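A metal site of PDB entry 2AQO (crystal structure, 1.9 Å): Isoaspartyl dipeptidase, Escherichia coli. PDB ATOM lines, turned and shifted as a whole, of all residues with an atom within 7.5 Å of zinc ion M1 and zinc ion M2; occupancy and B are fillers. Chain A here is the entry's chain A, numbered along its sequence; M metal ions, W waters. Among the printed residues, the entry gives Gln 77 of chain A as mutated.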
ATOM      1  N   HIS A  68     -20.495  -0.814 -21.928  1.00  0.00           N
ATOM      2  CA  HIS A  68     -21.806  -0.203 -22.041  1.00  0.00           C
ATOM      3  C   HIS A  68     -22.270   0.310 -20.708  1.00  0.00           C
ATOM      4  O   HIS A  68     -22.980  -0.359 -19.961  1.00  0.00           O
ATOM      5  CB  HIS A  68     -22.830  -1.243 -22.533  1.00  0.00           C
ATOM      6  CG  HIS A  68     -24.114  -0.617 -22.956  1.00  0.00           C
ATOM      7  ND1 HIS A  68     -24.577  -0.767 -24.242  1.00  0.00           N
ATOM      8  CD2 HIS A  68     -25.036   0.108 -22.260  1.00  0.00           C
ATOM      9  CE1 HIS A  68     -25.743  -0.149 -24.327  1.00  0.00           C
ATOM     10  NE2 HIS A  68     -26.017   0.395 -23.166  1.00  0.00           N
ATOM     11  N   VAL A  69     -21.837   1.521 -20.428  1.00  0.00           N
ATOM     12  CA  VAL A  69     -22.189   2.171 -19.176  1.00  0.00           C
ATOM     13  C   VAL A  69     -22.613   3.612 -19.372  1.00  0.00           C
ATOM     14  O   VAL A  69     -21.976   4.444 -20.048  1.00  0.00           O
ATOM     15  CB  VAL A  69     -20.976   2.203 -18.216  1.00  0.00           C
ATOM     16  CG1 VAL A  69     -21.386   2.789 -16.861  1.00  0.00           C
ATOM     17  CG2 VAL A  69     -20.319   0.832 -18.043  1.00  0.00           C
ATOM     18  N   HIS A  70     -23.690   3.955 -18.672  1.00  0.00           N
ATOM     19  CA  HIS A  70     -24.194   5.324 -18.662  1.00  0.00           C
ATOM     20  C   HIS A  70     -23.529   6.169 -17.586  1.00  0.00           C
ATOM     21  O   HIS A  70     -24.161   6.560 -16.577  1.00  0.00           O
ATOM     22  CB  HIS A  70     -25.717   5.380 -18.434  1.00  0.00           C
ATOM     23  CG  HIS A  70     -26.336   4.650 -19.585  1.00  0.00           C
ATOM     24  ND1 HIS A  70     -26.558   5.267 -20.809  1.00  0.00           N
ATOM     25  CD2 HIS A  70     -26.686   3.355 -19.679  1.00  0.00           C
ATOM     26  CE1 HIS A  70     -27.086   4.355 -21.590  1.00  0.00           C
ATOM     27  NE2 HIS A  70     -27.185   3.228 -20.932  1.00  0.00           N
ATOM     28  N   GLN A  77     -36.947   8.294 -19.193  1.00  0.00           N
ATOM     29  CA  GLN A  77     -38.039   7.756 -19.997  1.00  0.00           C
ATOM     30  C   GLN A  77     -39.395   7.942 -19.364  1.00  0.00           C
ATOM     31  O   GLN A  77     -40.383   7.769 -20.026  1.00  0.00           O
ATOM     32  CB  GLN A  77     -37.968   6.228 -20.268  1.00  0.00           C
ATOM     33  CG  GLN A  77     -36.875   5.787 -21.238  1.00  0.00           C
ATOM     34  CD  GLN A  77     -35.631   5.329 -20.524  1.00  0.00           C
ATOM     35  OE1 GLN A  77     -34.747   4.748 -21.303  1.00  0.00           O
ATOM     36  NE2 GLN A  77     -35.490   5.508 -19.329  1.00  0.00           N
ATOM     37  N   LEU A 103     -21.568   5.920 -22.693  1.00  0.00           N
ATOM     38  CA  LEU A 103     -22.480   6.235 -23.780  1.00  0.00           C
ATOM     39  C   LEU A 103     -23.776   6.843 -23.271  1.00  0.00           C
ATOM     40  O   LEU A 103     -24.069   6.825 -22.077  1.00  0.00           O
ATOM     41  CB  LEU A 103     -22.820   4.996 -24.692  1.00  0.00           C
ATOM     42  CG  LEU A 103     -23.058   3.648 -23.981  1.00  0.00           C
ATOM     43  CD1 LEU A 103     -24.252   3.677 -23.039  1.00  0.00           C
ATOM     44  CD2 LEU A 103     -23.310   2.601 -25.058  1.00  0.00           C
ATOM     45  N   LEU A 104     -24.528   7.378 -24.217  1.00  0.00           N
ATOM     46  CA  LEU A 104     -25.852   8.002 -24.019  1.00  0.00           C
ATOM     47  C   LEU A 104     -26.964   7.057 -24.528  1.00  0.00           C
ATOM     48  O   LEU A 104     -26.702   6.089 -25.299  1.00  0.00           O
ATOM     49  CB  LEU A 104     -25.951   9.394 -24.674  1.00  0.00           C
ATOM     50  CG  LEU A 104     -24.905  10.404 -24.211  1.00  0.00           C
ATOM     51  CD1 LEU A 104     -25.253  11.728 -24.901  1.00  0.00           C
ATOM     52  CD2 LEU A 104     -24.994  10.564 -22.672  1.00  0.00           C
ATOM     53  N   GLY A 105     -28.199   7.309 -24.103  1.00  0.00           N
ATOM     54  CA  GLY A 105     -29.324   6.472 -24.483  1.00  0.00           C
ATOM     55  C   GLY A 105     -30.456   7.260 -25.067  1.00  0.00           C
ATOM     56  O   GLY A 105     -30.357   8.066 -25.989  1.00  0.00           O
ATOM     57  N   THR A 106     -31.605   6.978 -24.495  1.00  0.00           N
ATOM     58  CA  THR A 106     -32.853   7.582 -24.951  1.00  0.00           C
ATOM     59  C   THR A 106     -32.796   9.113 -24.956  1.00  0.00           C
ATOM     60  O   THR A 106     -33.172   9.745 -25.913  1.00  0.00           O
ATOM     61  CB  THR A 106     -34.057   7.075 -24.107  1.00  0.00           C
ATOM     62  OG1 THR A 106     -34.018   5.663 -24.062  1.00  0.00           O
ATOM     63  CG2 THR A 106     -35.391   7.443 -24.758  1.00  0.00           C
ATOM     64  N   TYR A 137     -29.453   7.487 -28.824  1.00  0.00           N
ATOM     65  CA  TYR A 137     -30.428   6.753 -29.623  1.00  0.00           C
ATOM     66  C   TYR A 137     -30.780   7.483 -30.933  1.00  0.00           C
ATOM     67  O   TYR A 137     -31.039   6.879 -31.975  1.00  0.00           O
ATOM     68  CB  TYR A 137     -31.755   6.557 -28.905  1.00  0.00           C
ATOM     69  CG  TYR A 137     -31.857   5.455 -27.850  1.00  0.00           C
ATOM     70  CD1 TYR A 137     -30.721   4.892 -27.239  1.00  0.00           C
ATOM     71  CD2 TYR A 137     -33.127   5.033 -27.442  1.00  0.00           C
ATOM     72  CE1 TYR A 137     -30.856   3.872 -26.292  1.00  0.00           C
ATOM     73  CE2 TYR A 137     -33.273   4.038 -26.465  1.00  0.00           C
ATOM     74  CZ  TYR A 137     -32.134   3.504 -25.865  1.00  0.00           C
ATOM     75  OH  TYR A 137     -32.277   2.567 -24.863  1.00  0.00           O
ATOM     76  N   KCX A 162     -23.030   5.664 -31.190  1.00  0.00           N
ATOM     77  CA  KCX A 162     -24.126   4.837 -30.727  1.00  0.00           C
ATOM     78  CB  KCX A 162     -24.300   5.164 -29.229  1.00  0.00           C
ATOM     79  CG  KCX A 162     -25.653   4.731 -28.637  1.00  0.00           C
ATOM     80  CD  KCX A 162     -25.575   3.253 -28.288  1.00  0.00           C
ATOM     81  CE  KCX A 162     -26.816   2.696 -27.573  1.00  0.00           C
ATOM     82  NZ  KCX A 162     -27.164   3.443 -26.370  1.00  0.00           N
ATOM     83  C   KCX A 162     -25.407   5.262 -31.463  1.00  0.00           C
ATOM     84  O   KCX A 162     -25.500   6.404 -31.919  1.00  0.00           O
ATOM     85  CX  KCX A 162     -27.647   2.400 -25.486  1.00  0.00           C
ATOM     86  OQ1 KCX A 162     -27.881   1.248 -25.859  1.00  0.00           O
ATOM     87  OQ2 KCX A 162     -27.898   2.855 -24.289  1.00  0.00           O
ATOM     88  N   CYS A 163     -26.397   4.379 -31.517  1.00  0.00           N
ATOM     89  CA  CYS A 163     -27.735   4.583 -32.080  1.00  0.00           C
ATOM     90  C   CYS A 163     -28.713   3.520 -31.539  1.00  0.00           C
ATOM     91  O   CYS A 163     -28.331   2.580 -30.850  1.00  0.00           O
ATOM     92  CB  CYS A 163     -27.783   4.579 -33.623  1.00  0.00           C
ATOM     93  SG  CYS A 163     -27.555   2.922 -34.362  1.00  0.00           S
ATOM     94  N   ALA A 164     -29.992   3.668 -31.878  1.00  0.00           N
ATOM     95  CA  ALA A 164     -31.014   2.706 -31.495  1.00  0.00           C
ATOM     96  C   ALA A 164     -31.824   2.314 -32.722  1.00  0.00           C
ATOM     97  O   ALA A 164     -32.161   3.166 -33.558  1.00  0.00           O
ATOM     98  CB  ALA A 164     -31.938   3.307 -30.440  1.00  0.00           C
ATOM     99  N   ASP A 167     -36.878  -0.216 -32.051  1.00  0.00           N
ATOM    100  CA  ASP A 167     -37.276   0.108 -30.711  1.00  0.00           C
ATOM    101  C   ASP A 167     -38.297   1.237 -30.740  1.00  0.00           C
ATOM    102  O   ASP A 167     -38.173   2.157 -31.554  1.00  0.00           O
ATOM    103  CB  ASP A 167     -36.010   0.514 -29.939  1.00  0.00           C
ATOM    104  CG  ASP A 167     -36.268   0.752 -28.478  1.00  0.00           C
ATOM    105  OD1 ASP A 167     -36.821   1.739 -28.037  1.00  0.00           O
ATOM    106  OD2 ASP A 167     -35.869  -0.215 -27.729  1.00  0.00           O
ATOM    107  N   ARG A 169     -38.493   3.628 -28.974  1.00  0.00           N
ATOM    108  CA  ARG A 169     -37.820   4.848 -28.586  1.00  0.00           C
ATOM    109  C   ARG A 169     -36.841   5.310 -29.693  1.00  0.00           C
ATOM    110  O   ARG A 169     -36.048   6.225 -29.442  1.00  0.00           O
ATOM    111  CB  ARG A 169     -37.095   4.759 -27.265  1.00  0.00           C
ATOM    112  CG  ARG A 169     -38.052   4.638 -26.091  1.00  0.00           C
ATOM    113  CD  ARG A 169     -37.381   3.960 -24.891  1.00  0.00           C
ATOM    114  NE  ARG A 169     -36.827   2.672 -25.286  1.00  0.00           N
ATOM    115  CZ  ARG A 169     -36.046   1.883 -24.547  1.00  0.00           C
ATOM    116  NH1 ARG A 169     -35.671   2.197 -23.294  1.00  0.00           N
ATOM    117  NH2 ARG A 169     -35.632   0.727 -25.080  1.00  0.00           N
ATOM    118  N   PHE A 200     -25.452  -0.739 -31.910  1.00  0.00           N
ATOM    119  CA  PHE A 200     -26.891  -0.622 -32.035  1.00  0.00           C
ATOM    120  C   PHE A 200     -27.667  -1.137 -30.855  1.00  0.00           C
ATOM    121  O   PHE A 200     -27.685  -2.336 -30.616  1.00  0.00           O
ATOM    122  CB  PHE A 200     -27.379  -1.433 -33.231  1.00  0.00           C
ATOM    123  CG  PHE A 200     -26.711  -1.073 -34.535  1.00  0.00           C
ATOM    124  CD1 PHE A 200     -25.425  -1.529 -34.819  1.00  0.00           C
ATOM    125  CD2 PHE A 200     -27.387  -0.303 -35.489  1.00  0.00           C
ATOM    126  CE1 PHE A 200     -24.797  -1.192 -36.021  1.00  0.00           C
ATOM    127  CE2 PHE A 200     -26.789   0.012 -36.718  1.00  0.00           C
ATOM    128  CZ  PHE A 200     -25.475  -0.426 -36.965  1.00  0.00           C
ATOM    129  N   HIS A 201     -28.348  -0.222 -30.144  1.00  0.00           N
ATOM    130  CA  HIS A 201     -29.235  -0.584 -29.051  1.00  0.00           C
ATOM    131  C   HIS A 201     -30.392  -1.296 -29.764  1.00  0.00           C
ATOM    132  O   HIS A 201     -30.959  -0.769 -30.734  1.00  0.00           O
ATOM    133  CB  HIS A 201     -29.813   0.653 -28.304  1.00  0.00           C
ATOM    134  CG  HIS A 201     -31.157   0.384 -27.687  1.00  0.00           C
ATOM    135  ND1 HIS A 201     -31.292   0.058 -26.357  1.00  0.00           N
ATOM    136  CD2 HIS A 201     -32.394   0.329 -28.253  1.00  0.00           C
ATOM    137  CE1 HIS A 201     -32.572  -0.121 -26.109  1.00  0.00           C
ATOM    138  NE2 HIS A 201     -33.263   0.021 -27.233  1.00  0.00           N
ATOM    139  N   MET A 202     -30.713  -2.509 -29.363  1.00  0.00           N
ATOM    140  CA  MET A 202     -31.812  -3.208 -30.034  1.00  0.00           C
ATOM    141  C   MET A 202     -33.048  -3.161 -29.162  1.00  0.00           C
ATOM    142  O   MET A 202     -32.942  -3.364 -27.943  1.00  0.00           O
ATOM    143  CB  MET A 202     -31.515  -4.716 -30.230  1.00  0.00           C
ATOM    144  CG  MET A 202     -30.286  -4.991 -31.097  1.00  0.00           C
ATOM    145  SD  MET A 202     -30.294  -4.182 -32.732  1.00  0.00           S
ATOM    146  CE  MET A 202     -31.827  -4.809 -33.506  1.00  0.00           C
ATOM    147  N   GLY A 203     -34.200  -2.940 -29.749  1.00  0.00           N
ATOM    148  CA  GLY A 203     -35.398  -2.962 -28.939  1.00  0.00           C
ATOM    149  C   GLY A 203     -36.144  -4.255 -29.221  1.00  0.00           C
ATOM    150  O   GLY A 203     -35.567  -5.219 -29.701  1.00  0.00           O
ATOM    151  N   THR A 229     -26.355  -4.810 -29.427  1.00  0.00           N
ATOM    152  CA  THR A 229     -26.353  -5.014 -27.980  1.00  0.00           C
ATOM    153  C   THR A 229     -27.780  -5.312 -27.495  1.00  0.00           C
ATOM    154  O   THR A 229     -28.750  -5.101 -28.240  1.00  0.00           O
ATOM    155  CB  THR A 229     -25.640  -3.892 -27.200  1.00  0.00           C
ATOM    156  OG1 THR A 229     -25.539  -4.303 -25.856  1.00  0.00           O
ATOM    157  CG2 THR A 229     -26.460  -2.596 -27.255  1.00  0.00           C
ATOM    158  N   HIS A 230     -27.906  -5.847 -26.259  1.00  0.00           N
ATOM    159  CA  HIS A 230     -29.174  -6.259 -25.614  1.00  0.00           C
ATOM    160  C   HIS A 230     -29.789  -7.413 -26.438  1.00  0.00           C
ATOM    161  O   HIS A 230     -30.994  -7.502 -26.544  1.00  0.00           O
ATOM    162  CB  HIS A 230     -30.235  -5.134 -25.578  1.00  0.00           C
ATOM    163  CG  HIS A 230     -29.701  -3.804 -25.146  1.00  0.00           C
ATOM    164  ND1 HIS A 230     -28.809  -3.691 -24.101  1.00  0.00           N
ATOM    165  CD2 HIS A 230     -29.968  -2.562 -25.628  1.00  0.00           C
ATOM    166  CE1 HIS A 230     -28.525  -2.390 -23.965  1.00  0.00           C
ATOM    167  NE2 HIS A 230     -29.207  -1.699 -24.875  1.00  0.00           N
ATOM    168  N   ARG A 233     -32.610  -9.952 -25.021  1.00  0.00           N
ATOM    169  CA  ARG A 233     -33.863  -9.317 -24.645  1.00  0.00           C
ATOM    170  C   ARG A 233     -35.146 -10.004 -25.091  1.00  0.00           C
ATOM    171  O   ARG A 233     -36.197  -9.852 -24.462  1.00  0.00           O
ATOM    172  CB  ARG A 233     -33.818  -7.812 -24.985  1.00  0.00           C
ATOM    173  CG  ARG A 233     -33.875  -7.495 -26.489  1.00  0.00           C
ATOM    174  CD  ARG A 233     -34.066  -6.023 -26.824  1.00  0.00           C
ATOM    175  NE  ARG A 233     -35.025  -5.394 -25.911  1.00  0.00           N
ATOM    176  CZ  ARG A 233     -34.842  -4.278 -25.167  1.00  0.00           C
ATOM    177  NH1 ARG A 233     -33.750  -3.517 -25.171  1.00  0.00           N
ATOM    178  NH2 ARG A 233     -35.842  -3.948 -24.386  1.00  0.00           N
ATOM    179  N   THR A 254     -26.261  -8.368 -22.693  1.00  0.00           N
ATOM    180  CA  THR A 254     -26.402  -7.448 -21.578  1.00  0.00           C
ATOM    181  C   THR A 254     -26.604  -8.212 -20.299  1.00  0.00           C
ATOM    182  O   THR A 254     -27.588  -8.961 -20.175  1.00  0.00           O
ATOM    183  CB  THR A 254     -27.582  -6.501 -21.821  1.00  0.00           C
ATOM    184  OG1 THR A 254     -27.320  -5.788 -23.028  1.00  0.00           O
ATOM    185  CG2 THR A 254     -27.716  -5.534 -20.641  1.00  0.00           C
ATOM    186  N   SER A 284     -22.733  -4.342 -19.148  1.00  0.00           N
ATOM    187  CA  SER A 284     -23.771  -4.207 -18.145  1.00  0.00           C
ATOM    188  C   SER A 284     -25.011  -3.371 -18.427  1.00  0.00           C
ATOM    189  O   SER A 284     -26.095  -3.664 -17.910  1.00  0.00           O
ATOM    190  CB  SER A 284     -23.163  -3.713 -16.805  1.00  0.00           C
ATOM    191  OG  SER A 284     -22.654  -2.363 -16.882  1.00  0.00           O
ATOM    192  N   ASP A 285     -24.815  -2.286 -19.178  1.00  0.00           N
ATOM    193  CA  ASP A 285     -25.851  -1.305 -19.349  1.00  0.00           C
ATOM    194  C   ASP A 285     -26.030  -0.599 -17.976  1.00  0.00           C
ATOM    195  O   ASP A 285     -27.067  -0.001 -17.616  1.00  0.00           O
ATOM    196  CB  ASP A 285     -27.180  -1.827 -19.962  1.00  0.00           C
ATOM    197  CG  ASP A 285     -27.943  -0.667 -20.524  1.00  0.00           C
ATOM    198  OD1 ASP A 285     -27.433   0.426 -20.594  1.00  0.00           O
ATOM    199  OD2 ASP A 285     -29.170  -0.885 -20.876  1.00  0.00           O
ATOM    200  N   GLY A 286     -24.976  -0.665 -17.139  1.00  0.00           N
ATOM    201  CA  GLY A 286     -24.938  -0.089 -15.787  1.00  0.00           C
ATOM    202  C   GLY A 286     -25.340   1.406 -15.756  1.00  0.00           C
ATOM    203  O   GLY A 286     -25.062   2.192 -16.674  1.00  0.00           O
ATOM    204  N   ASN A 287     -26.037   1.764 -14.677  1.00  0.00           N
ATOM    205  CA  ASN A 287     -26.479   3.104 -14.453  1.00  0.00           C
ATOM    206  C   ASN A 287     -27.653   3.550 -15.320  1.00  0.00           C
ATOM    207  O   ASN A 287     -28.097   4.693 -15.299  1.00  0.00           O
ATOM    208  CB  ASN A 287     -25.329   4.114 -14.430  1.00  0.00           C
ATOM    209  CG  ASN A 287     -25.436   5.063 -13.283  1.00  0.00           C
ATOM    210  OD1 ASN A 287     -25.605   4.640 -12.134  1.00  0.00           O
ATOM    211  ND2 ASN A 287     -25.291   6.353 -13.641  1.00  0.00           N
ATOM    212  N   GLY A 288     -28.148   2.613 -16.103  1.00  0.00           N
ATOM    213  CA  GLY A 288     -29.312   2.928 -16.866  1.00  0.00           C
ATOM    214  C   GLY A 288     -30.454   2.791 -15.856  1.00  0.00           C
ATOM    215  O   GLY A 288     -30.280   2.372 -14.697  1.00  0.00           O
HETATM  216 ZN    ZN M   1     -29.842   0.379 -24.754  1.00  0.00          ZN
HETATM  217 ZN    ZN M   2     -27.726   1.608 -22.503  1.00  0.00          ZN
HETATM  218  O   HOH W   1     -30.665   1.800 -22.453  1.00  0.00           O
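A ring nitrogen (ND1) of His 230 lies within hydrogen-bond range of the side-chain hydroxyl (OG1) of Thr 254 (2.8 Å).
OH of Tyr 137 lies close to ND1 of His 201 (3.1 Å).
NE2 of His 201 lies within hydrogen-bond range of NH2 of Arg 169 (3.3 Å).
The backbone NH of His 201 sits at hydrogen-bond distance from the backbone carbonyl oxygen of Cys 163, at 2.9 Å.
The backbone carbonyl oxygen (O) of His 68 is in hydrogen-bond range of the backbone NH (N) of Gly 286, at 3.5 Å.
O of Leu 103 is in hydrogen-bond range of ND1 of His 70 (3.2 Å).
N of Tyr 137 sits at hydrogen-bond distance from O of Gly 105.
The backbone carbonyl oxygen of Tyr 137 is in hydrogen-bond range of the backbone NH of Ala 164 (3.4 Å).
OH of Tyr 137 touches zinc ion M1, at 3.3 Å.
Of the 27 residues printed, 4 come within 4 Å of zinc ion M1.
The nearest printed residue that does not touch zinc ion M1 is Asp 285 (4.1 Å).
Within 4 Å of zinc ion M2: His 68, His 70, KCX 162 and Asp 285.
The nearest printed residue that does not touch zinc ion M2 is Leu 103 (4.1 Å).
A ring nitrogen (NE2) of His 230 binds zinc ion M1, at 2.2 Å.
Zinc ion M1 is bound by ND1 of His 201, 2.2 Å away.
OQ1 of KCX 162 is bound to zinc ion M1 (2.4 Å).
Slightly farther from zinc ion M1 lies water W1 (2.8 Å).
Zinc ion M2 is bound by OQ2 of KCX 162 (2.2 Å), NE2 of His 68 (2.2 Å), OD1 of Asp 285 (2.3 Å) and NE2 of His 70 (2.3 Å).
Water W1 lies within hydrogen-bond range of OH of Tyr 137 (3.0 Å) and OD2 of Asp 285 (3.5 Å).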
